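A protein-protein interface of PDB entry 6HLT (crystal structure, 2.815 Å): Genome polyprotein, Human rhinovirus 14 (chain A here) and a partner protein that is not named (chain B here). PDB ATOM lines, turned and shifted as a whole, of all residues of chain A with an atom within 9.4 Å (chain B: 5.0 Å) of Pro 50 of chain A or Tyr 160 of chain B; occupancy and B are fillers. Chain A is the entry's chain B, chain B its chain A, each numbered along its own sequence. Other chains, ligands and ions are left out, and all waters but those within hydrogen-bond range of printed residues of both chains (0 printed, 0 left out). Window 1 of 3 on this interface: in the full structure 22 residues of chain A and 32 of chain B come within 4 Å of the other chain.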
ATOM      1  N   PRO A  47     -21.075 -12.489  -7.475  1.00  0.00           N
ATOM      2  CA  PRO A  47     -20.047 -12.339  -6.436  1.00  0.00           C
ATOM      3  C   PRO A  47     -18.860 -11.491  -6.901  1.00  0.00           C
ATOM      4  O   PRO A  47     -18.365 -11.631  -8.025  1.00  0.00           O
ATOM      5  CB  PRO A  47     -19.627 -13.791  -6.136  1.00  0.00           C
ATOM      6  CG  PRO A  47     -20.104 -14.593  -7.269  1.00  0.00           C
ATOM      7  CD  PRO A  47     -21.331 -13.903  -7.782  1.00  0.00           C
ATOM      8  N   GLU A  48     -18.426 -10.601  -6.014  1.00  0.00           N
ATOM      9  CA  GLU A  48     -17.389  -9.617  -6.309  1.00  0.00           C
ATOM     10  C   GLU A  48     -16.036 -10.056  -5.757  1.00  0.00           C
ATOM     11  O   GLU A  48     -15.965 -10.752  -4.740  1.00  0.00           O
ATOM     12  CB  GLU A  48     -17.787  -8.260  -5.730  1.00  0.00           C
ATOM     13  CG  GLU A  48     -16.824  -7.136  -6.031  1.00  0.00           C
ATOM     14  CD  GLU A  48     -16.774  -6.783  -7.497  1.00  0.00           C
ATOM     15  OE1 GLU A  48     -15.827  -7.233  -8.176  1.00  0.00           O
ATOM     16  OE2 GLU A  48     -17.671  -6.046  -7.965  1.00  0.00           O
ATOM     17  N   ILE A  49     -14.975  -9.697  -6.477  1.00  0.00           N
ATOM     18  CA  ILE A  49     -13.603 -10.025  -6.087  1.00  0.00           C
ATOM     19  C   ILE A  49     -12.790  -8.745  -5.890  1.00  0.00           C
ATOM     20  O   ILE A  49     -12.457  -8.075  -6.872  1.00  0.00           O
ATOM     21  CB  ILE A  49     -12.930 -10.925  -7.150  1.00  0.00           C
ATOM     22  CG1 ILE A  49     -13.784 -12.178  -7.377  1.00  0.00           C
ATOM     23  CG2 ILE A  49     -11.521 -11.320  -6.720  1.00  0.00           C
ATOM     24  CD1 ILE A  49     -13.417 -12.979  -8.598  1.00  0.00           C
ATOM     25  N   PRO A  50     -12.452  -8.401  -4.630  1.00  0.00           N
ATOM     26  CA  PRO A  50     -11.690  -7.162  -4.445  1.00  0.00           C
ATOM     27  C   PRO A  50     -10.287  -7.261  -4.992  1.00  0.00           C
ATOM     28  O   PRO A  50      -9.767  -8.370  -5.149  1.00  0.00           O
ATOM     29  CB  PRO A  50     -11.650  -6.991  -2.921  1.00  0.00           C
ATOM     30  CG  PRO A  50     -12.754  -7.811  -2.411  1.00  0.00           C
ATOM     31  CD  PRO A  50     -12.830  -8.984  -3.334  1.00  0.00           C
ATOM     32  N   THR A  51      -9.677  -6.112  -5.261  1.00  0.00           N
ATOM     33  CA  THR A  51      -8.326  -6.128  -5.761  1.00  0.00           C
ATOM     34  C   THR A  51      -7.338  -6.086  -4.617  1.00  0.00           C
ATOM     35  O   THR A  51      -6.816  -7.115  -4.192  1.00  0.00           O
ATOM     36  CB  THR A  51      -8.043  -4.942  -6.689  1.00  0.00           C
ATOM     37  OG1 THR A  51      -8.627  -3.754  -6.145  1.00  0.00           O
ATOM     38  CG2 THR A  51      -8.621  -5.195  -8.072  1.00  0.00           C
ATOM     39  N   ASN A  52      -7.152  -4.903  -4.060  1.00  0.00           N
ATOM     40  CA  ASN A  52      -6.110  -4.702  -3.073  1.00  0.00           C
ATOM     41  C   ASN A  52      -6.728  -4.505  -1.718  1.00  0.00           C
ATOM     42  O   ASN A  52      -7.840  -3.992  -1.601  1.00  0.00           O
ATOM     43  CB  ASN A  52      -5.237  -3.502  -3.435  1.00  0.00           C
ATOM     44  CG  ASN A  52      -4.314  -3.790  -4.600  1.00  0.00           C
ATOM     45  OD1 ASN A  52      -4.671  -3.569  -5.756  1.00  0.00           O
ATOM     46  ND2 ASN A  52      -3.123  -4.285  -4.304  1.00  0.00           N
ATOM     47  N   ILE A  53      -6.014  -4.952  -0.696  1.00  0.00           N
ATOM     48  CA  ILE A  53      -6.421  -4.687   0.658  1.00  0.00           C
ATOM     49  C   ILE A  53      -5.248  -4.031   1.365  1.00  0.00           C
ATOM     50  O   ILE A  53      -4.242  -4.673   1.666  1.00  0.00           O
ATOM     51  CB  ILE A  53      -6.883  -5.971   1.347  1.00  0.00           C
ATOM     52  CG1 ILE A  53      -8.012  -6.594   0.507  1.00  0.00           C
ATOM     53  CG2 ILE A  53      -7.312  -5.670   2.779  1.00  0.00           C
ATOM     54  CD1 ILE A  53      -8.774  -7.715   1.173  1.00  0.00           C
ATOM     55  N   GLU A  54      -5.427  -2.747   1.661  1.00  0.00           N
ATOM     56  CA  GLU A  54      -4.356  -1.872   2.125  1.00  0.00           C
ATOM     57  C   GLU A  54      -4.454  -1.761   3.638  1.00  0.00           C
ATOM     58  O   GLU A  54      -5.540  -1.905   4.199  1.00  0.00           O
ATOM     59  CB  GLU A  54      -4.449  -0.485   1.461  1.00  0.00           C
ATOM     60  CG  GLU A  54      -4.859  -0.529  -0.015  1.00  0.00           C
ATOM     61  CD  GLU A  54      -4.767   0.827  -0.722  1.00  0.00           C
ATOM     62  OE1 GLU A  54      -4.041   0.909  -1.742  1.00  0.00           O
ATOM     63  OE2 GLU A  54      -5.427   1.798  -0.279  1.00  0.00           O
ATOM     64  N   PHE B  21     -24.462 -15.510   8.929  1.00  0.00           N
ATOM     65  CA  PHE B  21     -23.530 -14.816   8.046  1.00  0.00           C
ATOM     66  C   PHE B  21     -22.104 -15.323   8.260  1.00  0.00           C
ATOM     67  O   PHE B  21     -21.483 -15.829   7.328  1.00  0.00           O
ATOM     68  CB  PHE B  21     -23.613 -13.301   8.276  1.00  0.00           C
ATOM     69  CG  PHE B  21     -22.711 -12.490   7.381  1.00  0.00           C
ATOM     70  CD1 PHE B  21     -22.916 -12.451   6.012  1.00  0.00           C
ATOM     71  CD2 PHE B  21     -21.667 -11.750   7.916  1.00  0.00           C
ATOM     72  CE1 PHE B  21     -22.088 -11.702   5.192  1.00  0.00           C
ATOM     73  CE2 PHE B  21     -20.841 -11.000   7.104  1.00  0.00           C
ATOM     74  CZ  PHE B  21     -21.050 -10.975   5.743  1.00  0.00           C
ATOM     75  N   ILE B  25     -19.671 -17.323   5.664  1.00  0.00           N
ATOM     76  CA  ILE B  25     -18.372 -16.763   5.263  1.00  0.00           C
ATOM     77  C   ILE B  25     -17.247 -17.781   5.405  1.00  0.00           C
ATOM     78  O   ILE B  25     -16.516 -18.034   4.454  1.00  0.00           O
ATOM     79  CB  ILE B  25     -18.006 -15.503   6.103  1.00  0.00           C
ATOM     80  CG1 ILE B  25     -18.956 -14.341   5.803  1.00  0.00           C
ATOM     81  CG2 ILE B  25     -16.561 -15.055   5.857  1.00  0.00           C
ATOM     82  CD1 ILE B  25     -18.925 -13.819   4.371  1.00  0.00           C
ATOM     83  N   SER B  31     -12.064 -15.489   4.020  1.00  0.00           N
ATOM     84  CA  SER B  31     -11.747 -14.077   4.004  1.00  0.00           C
ATOM     85  C   SER B  31     -12.306 -13.478   5.269  1.00  0.00           C
ATOM     86  O   SER B  31     -13.488 -13.133   5.345  1.00  0.00           O
ATOM     87  CB  SER B  31     -12.351 -13.391   2.785  1.00  0.00           C
ATOM     88  OG  SER B  31     -13.747 -13.633   2.725  1.00  0.00           O
ATOM     89  N   ILE B  33     -10.930 -10.423   7.725  1.00  0.00           N
ATOM     90  CA  ILE B  33      -9.893  -9.441   7.916  1.00  0.00           C
ATOM     91  C   ILE B  33      -9.730  -9.232   9.413  1.00  0.00           C
ATOM     92  O   ILE B  33     -10.712  -9.050  10.127  1.00  0.00           O
ATOM     93  CB  ILE B  33     -10.228  -8.129   7.186  1.00  0.00           C
ATOM     94  CG1 ILE B  33     -10.299  -8.393   5.673  1.00  0.00           C
ATOM     95  CG2 ILE B  33      -9.188  -7.064   7.506  1.00  0.00           C
ATOM     96  CD1 ILE B  33     -10.628  -7.177   4.810  1.00  0.00           C
ATOM     97  N   VAL B  43     -10.500  -2.018   1.701  1.00  0.00           N
ATOM     98  CA  VAL B  43     -10.747  -2.999   0.649  1.00  0.00           C
ATOM     99  C   VAL B  43     -11.128  -2.254  -0.624  1.00  0.00           C
ATOM    100  O   VAL B  43     -12.147  -1.563  -0.663  1.00  0.00           O
ATOM    101  CB  VAL B  43     -11.863  -4.002   1.031  1.00  0.00           C
ATOM    102  CG1 VAL B  43     -12.005  -5.059  -0.027  1.00  0.00           C
ATOM    103  CG2 VAL B  43     -11.560  -4.675   2.351  1.00  0.00           C
ATOM    104  N   ARG B  44     -10.291  -2.380  -1.654  1.00  0.00           N
ATOM    105  CA  ARG B  44     -10.538  -1.725  -2.937  1.00  0.00           C
ATOM    106  C   ARG B  44     -11.379  -2.647  -3.804  1.00  0.00           C
ATOM    107  O   ARG B  44     -11.046  -3.818  -3.996  1.00  0.00           O
ATOM    108  CB  ARG B  44      -9.232  -1.371  -3.655  1.00  0.00           C
ATOM    109  CG  ARG B  44      -8.240  -0.581  -2.818  1.00  0.00           C
ATOM    110  CD  ARG B  44      -7.029  -0.164  -3.635  1.00  0.00           C
ATOM    111  NE  ARG B  44      -7.314   1.003  -4.464  1.00  0.00           N
ATOM    112  CZ  ARG B  44      -7.190   2.264  -4.054  1.00  0.00           C
ATOM    113  NH1 ARG B  44      -6.779   2.554  -2.818  1.00  0.00           N
ATOM    114  NH2 ARG B  44      -7.479   3.246  -4.887  1.00  0.00           N
ATOM    115  N   VAL B  45     -12.493  -2.113  -4.296  1.00  0.00           N
ATOM    116  CA  VAL B  45     -13.445  -2.876  -5.090  1.00  0.00           C
ATOM    117  C   VAL B  45     -13.772  -2.112  -6.366  1.00  0.00           C
ATOM    118  O   VAL B  45     -14.607  -1.207  -6.355  1.00  0.00           O
ATOM    119  CB  VAL B  45     -14.730  -3.163  -4.314  1.00  0.00           C
ATOM    120  CG1 VAL B  45     -15.622  -4.092  -5.126  1.00  0.00           C
ATOM    121  CG2 VAL B  45     -14.397  -3.755  -2.933  1.00  0.00           C
ATOM    122  N   PRO B  46     -13.073  -2.430  -7.462  1.00  0.00           N
ATOM    123  CA  PRO B  46     -13.315  -1.690  -8.705  1.00  0.00           C
ATOM    124  C   PRO B  46     -14.698  -1.938  -9.322  1.00  0.00           C
ATOM    125  O   PRO B  46     -15.365  -2.931  -9.011  1.00  0.00           O
ATOM    126  CB  PRO B  46     -12.197  -2.188  -9.628  1.00  0.00           C
ATOM    127  CG  PRO B  46     -11.798  -3.507  -9.084  1.00  0.00           C
ATOM    128  CD  PRO B  46     -12.007  -3.439  -7.611  1.00  0.00           C
ATOM    129  N   GLU B  57     -21.643  -6.314   2.509  1.00  0.00           N
ATOM    130  CA  GLU B  57     -22.079  -6.798   3.811  1.00  0.00           C
ATOM    131  C   GLU B  57     -20.873  -6.903   4.730  1.00  0.00           C
ATOM    132  O   GLU B  57     -19.797  -7.295   4.289  1.00  0.00           O
ATOM    133  CB  GLU B  57     -22.746  -8.162   3.699  1.00  0.00           C
ATOM    134  CG  GLU B  57     -23.972  -8.189   2.830  1.00  0.00           C
ATOM    135  CD  GLU B  57     -24.315  -9.590   2.386  1.00  0.00           C
ATOM    136  OE1 GLU B  57     -23.385 -10.390   2.178  1.00  0.00           O
ATOM    137  OE2 GLU B  57     -25.509  -9.902   2.253  1.00  0.00           O
ATOM    138  N   PHE B  58     -21.043  -6.574   6.005  1.00  0.00           N
ATOM    139  CA  PHE B  58     -19.965  -6.787   6.955  1.00  0.00           C
ATOM    140  C   PHE B  58     -20.491  -7.021   8.367  1.00  0.00           C
ATOM    141  O   PHE B  58     -21.612  -6.631   8.708  1.00  0.00           O
ATOM    142  CB  PHE B  58     -18.979  -5.607   6.928  1.00  0.00           C
ATOM    143  CG  PHE B  58     -19.565  -4.296   7.352  1.00  0.00           C
ATOM    144  CD1 PHE B  58     -20.196  -3.475   6.439  1.00  0.00           C
ATOM    145  CD2 PHE B  58     -19.452  -3.874   8.655  1.00  0.00           C
ATOM    146  CE1 PHE B  58     -20.723  -2.264   6.826  1.00  0.00           C
ATOM    147  CE2 PHE B  58     -19.972  -2.666   9.052  1.00  0.00           C
ATOM    148  CZ  PHE B  58     -20.610  -1.859   8.139  1.00  0.00           C
ATOM    149  N   PHE B 146     -12.494  -0.059   6.703  1.00  0.00           N
ATOM    150  CA  PHE B 146     -12.740  -0.575   8.041  1.00  0.00           C
ATOM    151  C   PHE B 146     -11.738   0.080   8.998  1.00  0.00           C
ATOM    152  O   PHE B 146     -10.543  -0.234   8.992  1.00  0.00           O
ATOM    153  CB  PHE B 146     -12.633  -2.105   8.055  1.00  0.00           C
ATOM    154  CG  PHE B 146     -13.581  -2.789   7.089  1.00  0.00           C
ATOM    155  CD1 PHE B 146     -14.901  -3.053   7.444  1.00  0.00           C
ATOM    156  CD2 PHE B 146     -13.155  -3.152   5.821  1.00  0.00           C
ATOM    157  CE1 PHE B 146     -15.765  -3.671   6.554  1.00  0.00           C
ATOM    158  CE2 PHE B 146     -14.017  -3.773   4.926  1.00  0.00           C
ATOM    159  CZ  PHE B 146     -15.319  -4.032   5.294  1.00  0.00           C
ATOM    160  N   VAL B 158     -13.170  -8.998  11.169  1.00  0.00           N
ATOM    161  CA  VAL B 158     -14.125  -8.503  10.184  1.00  0.00           C
ATOM    162  C   VAL B 158     -14.458  -9.563   9.145  1.00  0.00           C
ATOM    163  O   VAL B 158     -13.593 -10.004   8.390  1.00  0.00           O
ATOM    164  CB  VAL B 158     -13.583  -7.246   9.462  1.00  0.00           C
ATOM    165  CG1 VAL B 158     -14.491  -6.827   8.291  1.00  0.00           C
ATOM    166  CG2 VAL B 158     -13.425  -6.105  10.448  1.00  0.00           C
ATOM    167  N   TYR B 159     -15.727  -9.962   9.130  1.00  0.00           N
ATOM    168  CA  TYR B 159     -16.278 -10.815   8.088  1.00  0.00           C
ATOM    169  C   TYR B 159     -17.017  -9.933   7.096  1.00  0.00           C
ATOM    170  O   TYR B 159     -17.895  -9.172   7.494  1.00  0.00           O
ATOM    171  CB  TYR B 159     -17.237 -11.852   8.669  1.00  0.00           C
ATOM    172  CG  TYR B 159     -16.693 -12.652   9.829  1.00  0.00           C
ATOM    173  CD1 TYR B 159     -16.597 -12.096  11.101  1.00  0.00           C
ATOM    174  CD2 TYR B 159     -16.308 -13.973   9.659  1.00  0.00           C
ATOM    175  CE1 TYR B 159     -16.113 -12.830  12.166  1.00  0.00           C
ATOM    176  CE2 TYR B 159     -15.824 -14.714  10.718  1.00  0.00           C
ATOM    177  CZ  TYR B 159     -15.730 -14.137  11.971  1.00  0.00           C
ATOM    178  OH  TYR B 159     -15.250 -14.871  13.031  1.00  0.00           O
ATOM    179  N   TYR B 160     -16.674 -10.024   5.815  1.00  0.00           N
ATOM    180  CA  TYR B 160     -17.330  -9.184   4.816  1.00  0.00           C
ATOM    181  C   TYR B 160     -17.647  -9.964   3.542  1.00  0.00           C
ATOM    182  O   TYR B 160     -17.039 -11.001   3.265  1.00  0.00           O
ATOM    183  CB  TYR B 160     -16.465  -7.950   4.495  1.00  0.00           C
ATOM    184  CG  TYR B 160     -15.283  -8.200   3.593  1.00  0.00           C
ATOM    185  CD1 TYR B 160     -14.083  -8.660   4.107  1.00  0.00           C
ATOM    186  CD2 TYR B 160     -15.365  -7.962   2.228  1.00  0.00           C
ATOM    187  CE1 TYR B 160     -12.995  -8.890   3.290  1.00  0.00           C
ATOM    188  CE2 TYR B 160     -14.279  -8.187   1.397  1.00  0.00           C
ATOM    189  CZ  TYR B 160     -13.092  -8.652   1.936  1.00  0.00           C
ATOM    190  OH  TYR B 160     -11.988  -8.888   1.141  1.00  0.00           O
ATOM    191  N   ARG B 161     -18.620  -9.451   2.793  1.00  0.00           N
ATOM    192  CA  ARG B 161     -19.030 -10.026   1.519  1.00  0.00           C
ATOM    193  C   ARG B 161     -19.424  -8.910   0.552  1.00  0.00           C
ATOM    194  O   ARG B 161     -20.079  -7.942   0.938  1.00  0.00           O
ATOM    195  CB  ARG B 161     -20.200 -11.000   1.717  1.00  0.00           C
ATOM    196  CG  ARG B 161     -20.327 -12.041   0.609  1.00  0.00           C
ATOM    197  CD  ARG B 161     -21.747 -12.580   0.470  1.00  0.00           C
ATOM    198  NE  ARG B 161     -22.209 -13.328   1.638  1.00  0.00           N
ATOM    199  CZ  ARG B 161     -23.484 -13.597   1.905  1.00  0.00           C
ATOM    200  NH1 ARG B 161     -24.441 -13.178   1.094  1.00  0.00           N
ATOM    201  NH2 ARG B 161     -23.808 -14.280   2.991  1.00  0.00           N
ATOM    202  N   VAL B 162     -19.031  -9.051  -0.707  1.00  0.00           N
ATOM    203  CA  VAL B 162     -19.301  -8.024  -1.705  1.00  0.00           C
ATOM    204  C   VAL B 162     -19.963  -8.636  -2.932  1.00  0.00           C
ATOM    205  O   VAL B 162     -19.670  -9.770  -3.315  1.00  0.00           O
ATOM    206  CB  VAL B 162     -18.008  -7.293  -2.124  1.00  0.00           C
ATOM    207  CG1 VAL B 162     -18.318  -6.116  -3.010  1.00  0.00           C
ATOM    208  CG2 VAL B 162     -17.276  -6.798  -0.907  1.00  0.00           C
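The backbone NH (N) of Thr 51 of chain A lies within hydrogen-bond range of the backbone carbonyl oxygen (O) of Arg 44 of chain B, at 3.0 Å.
The backbone carbonyl oxygen of Asn 52 of chain A sits at hydrogen-bond distance from the backbone NH of Arg 44 of chain B (2.9 Å).
NH1 of Arg 44 of chain B lies within salt-bridge range of OE2 of Glu 54 of chain A, 3.0 Å away.
The backbone carbonyl oxygen of Val 162 of chain B sits at hydrogen-bond distance from the backbone NH of Glu 48 of chain A, at 3.1 Å.
Val 45 of chain B touches Glu 48 of chain A.
CG1 of Val 43 of chain B touches CB of Pro 50 of chain A (3.5 Å).
Arg 44 of chain B touches Pro 50 of chain A (O to CB, 3.4 Å).
Pro 50 of chain A touches Tyr 160 of chain B (CG to OH, 3.8 Å).
Thr 51 of chain A touches Pro 46 of chain B (OG1 to CD, 3.7 Å).
Asn 52 of chain A touches Val 43 of chain B (O to CA, 3.8 Å).
Tyr 160 of chain B touches Ile 53 of chain A.
Of chain B, only Val 43, Arg 44 and Tyr 160 come within 4 Å of Pro 50 of chain A.
Of the printed residues of chain B, Ile 53 of chain A touches Tyr 160 (3.4 Å).
Of the printed residues of chain B, Glu 54 of chain A touches Arg 44 (3.0 Å).
Printed residues of chain A within 4 Å of Val 45 of chain B: Glu 48.
Of chain A, only Pro 50 and Ile 53 come within 4 Å of Tyr 160 of chain B.
Printed residues of chain A within 4 Å of Val 162 of chain B: Glu 48.
The nearest residue of chain B that does not touch Pro 50 of chain A is Val 45 of chain B (4.2 Å).
Printed residues of chain A that touch a printed residue of chain B: Glu 48, Pro 50, Thr 51, Asn 52, Ile 53 and Glu 54.
Hydrophobic or aromatic side chains of chain A that line the printed part of chain B: Pro 50 and Ile 53.
Among the printed residues, Asp or Glu carboxylates within 4 Å of a Lys or Arg side-chain nitrogen of the other chain: Glu 54 of chain A with Arg 44 of chain B (3.0 Å).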
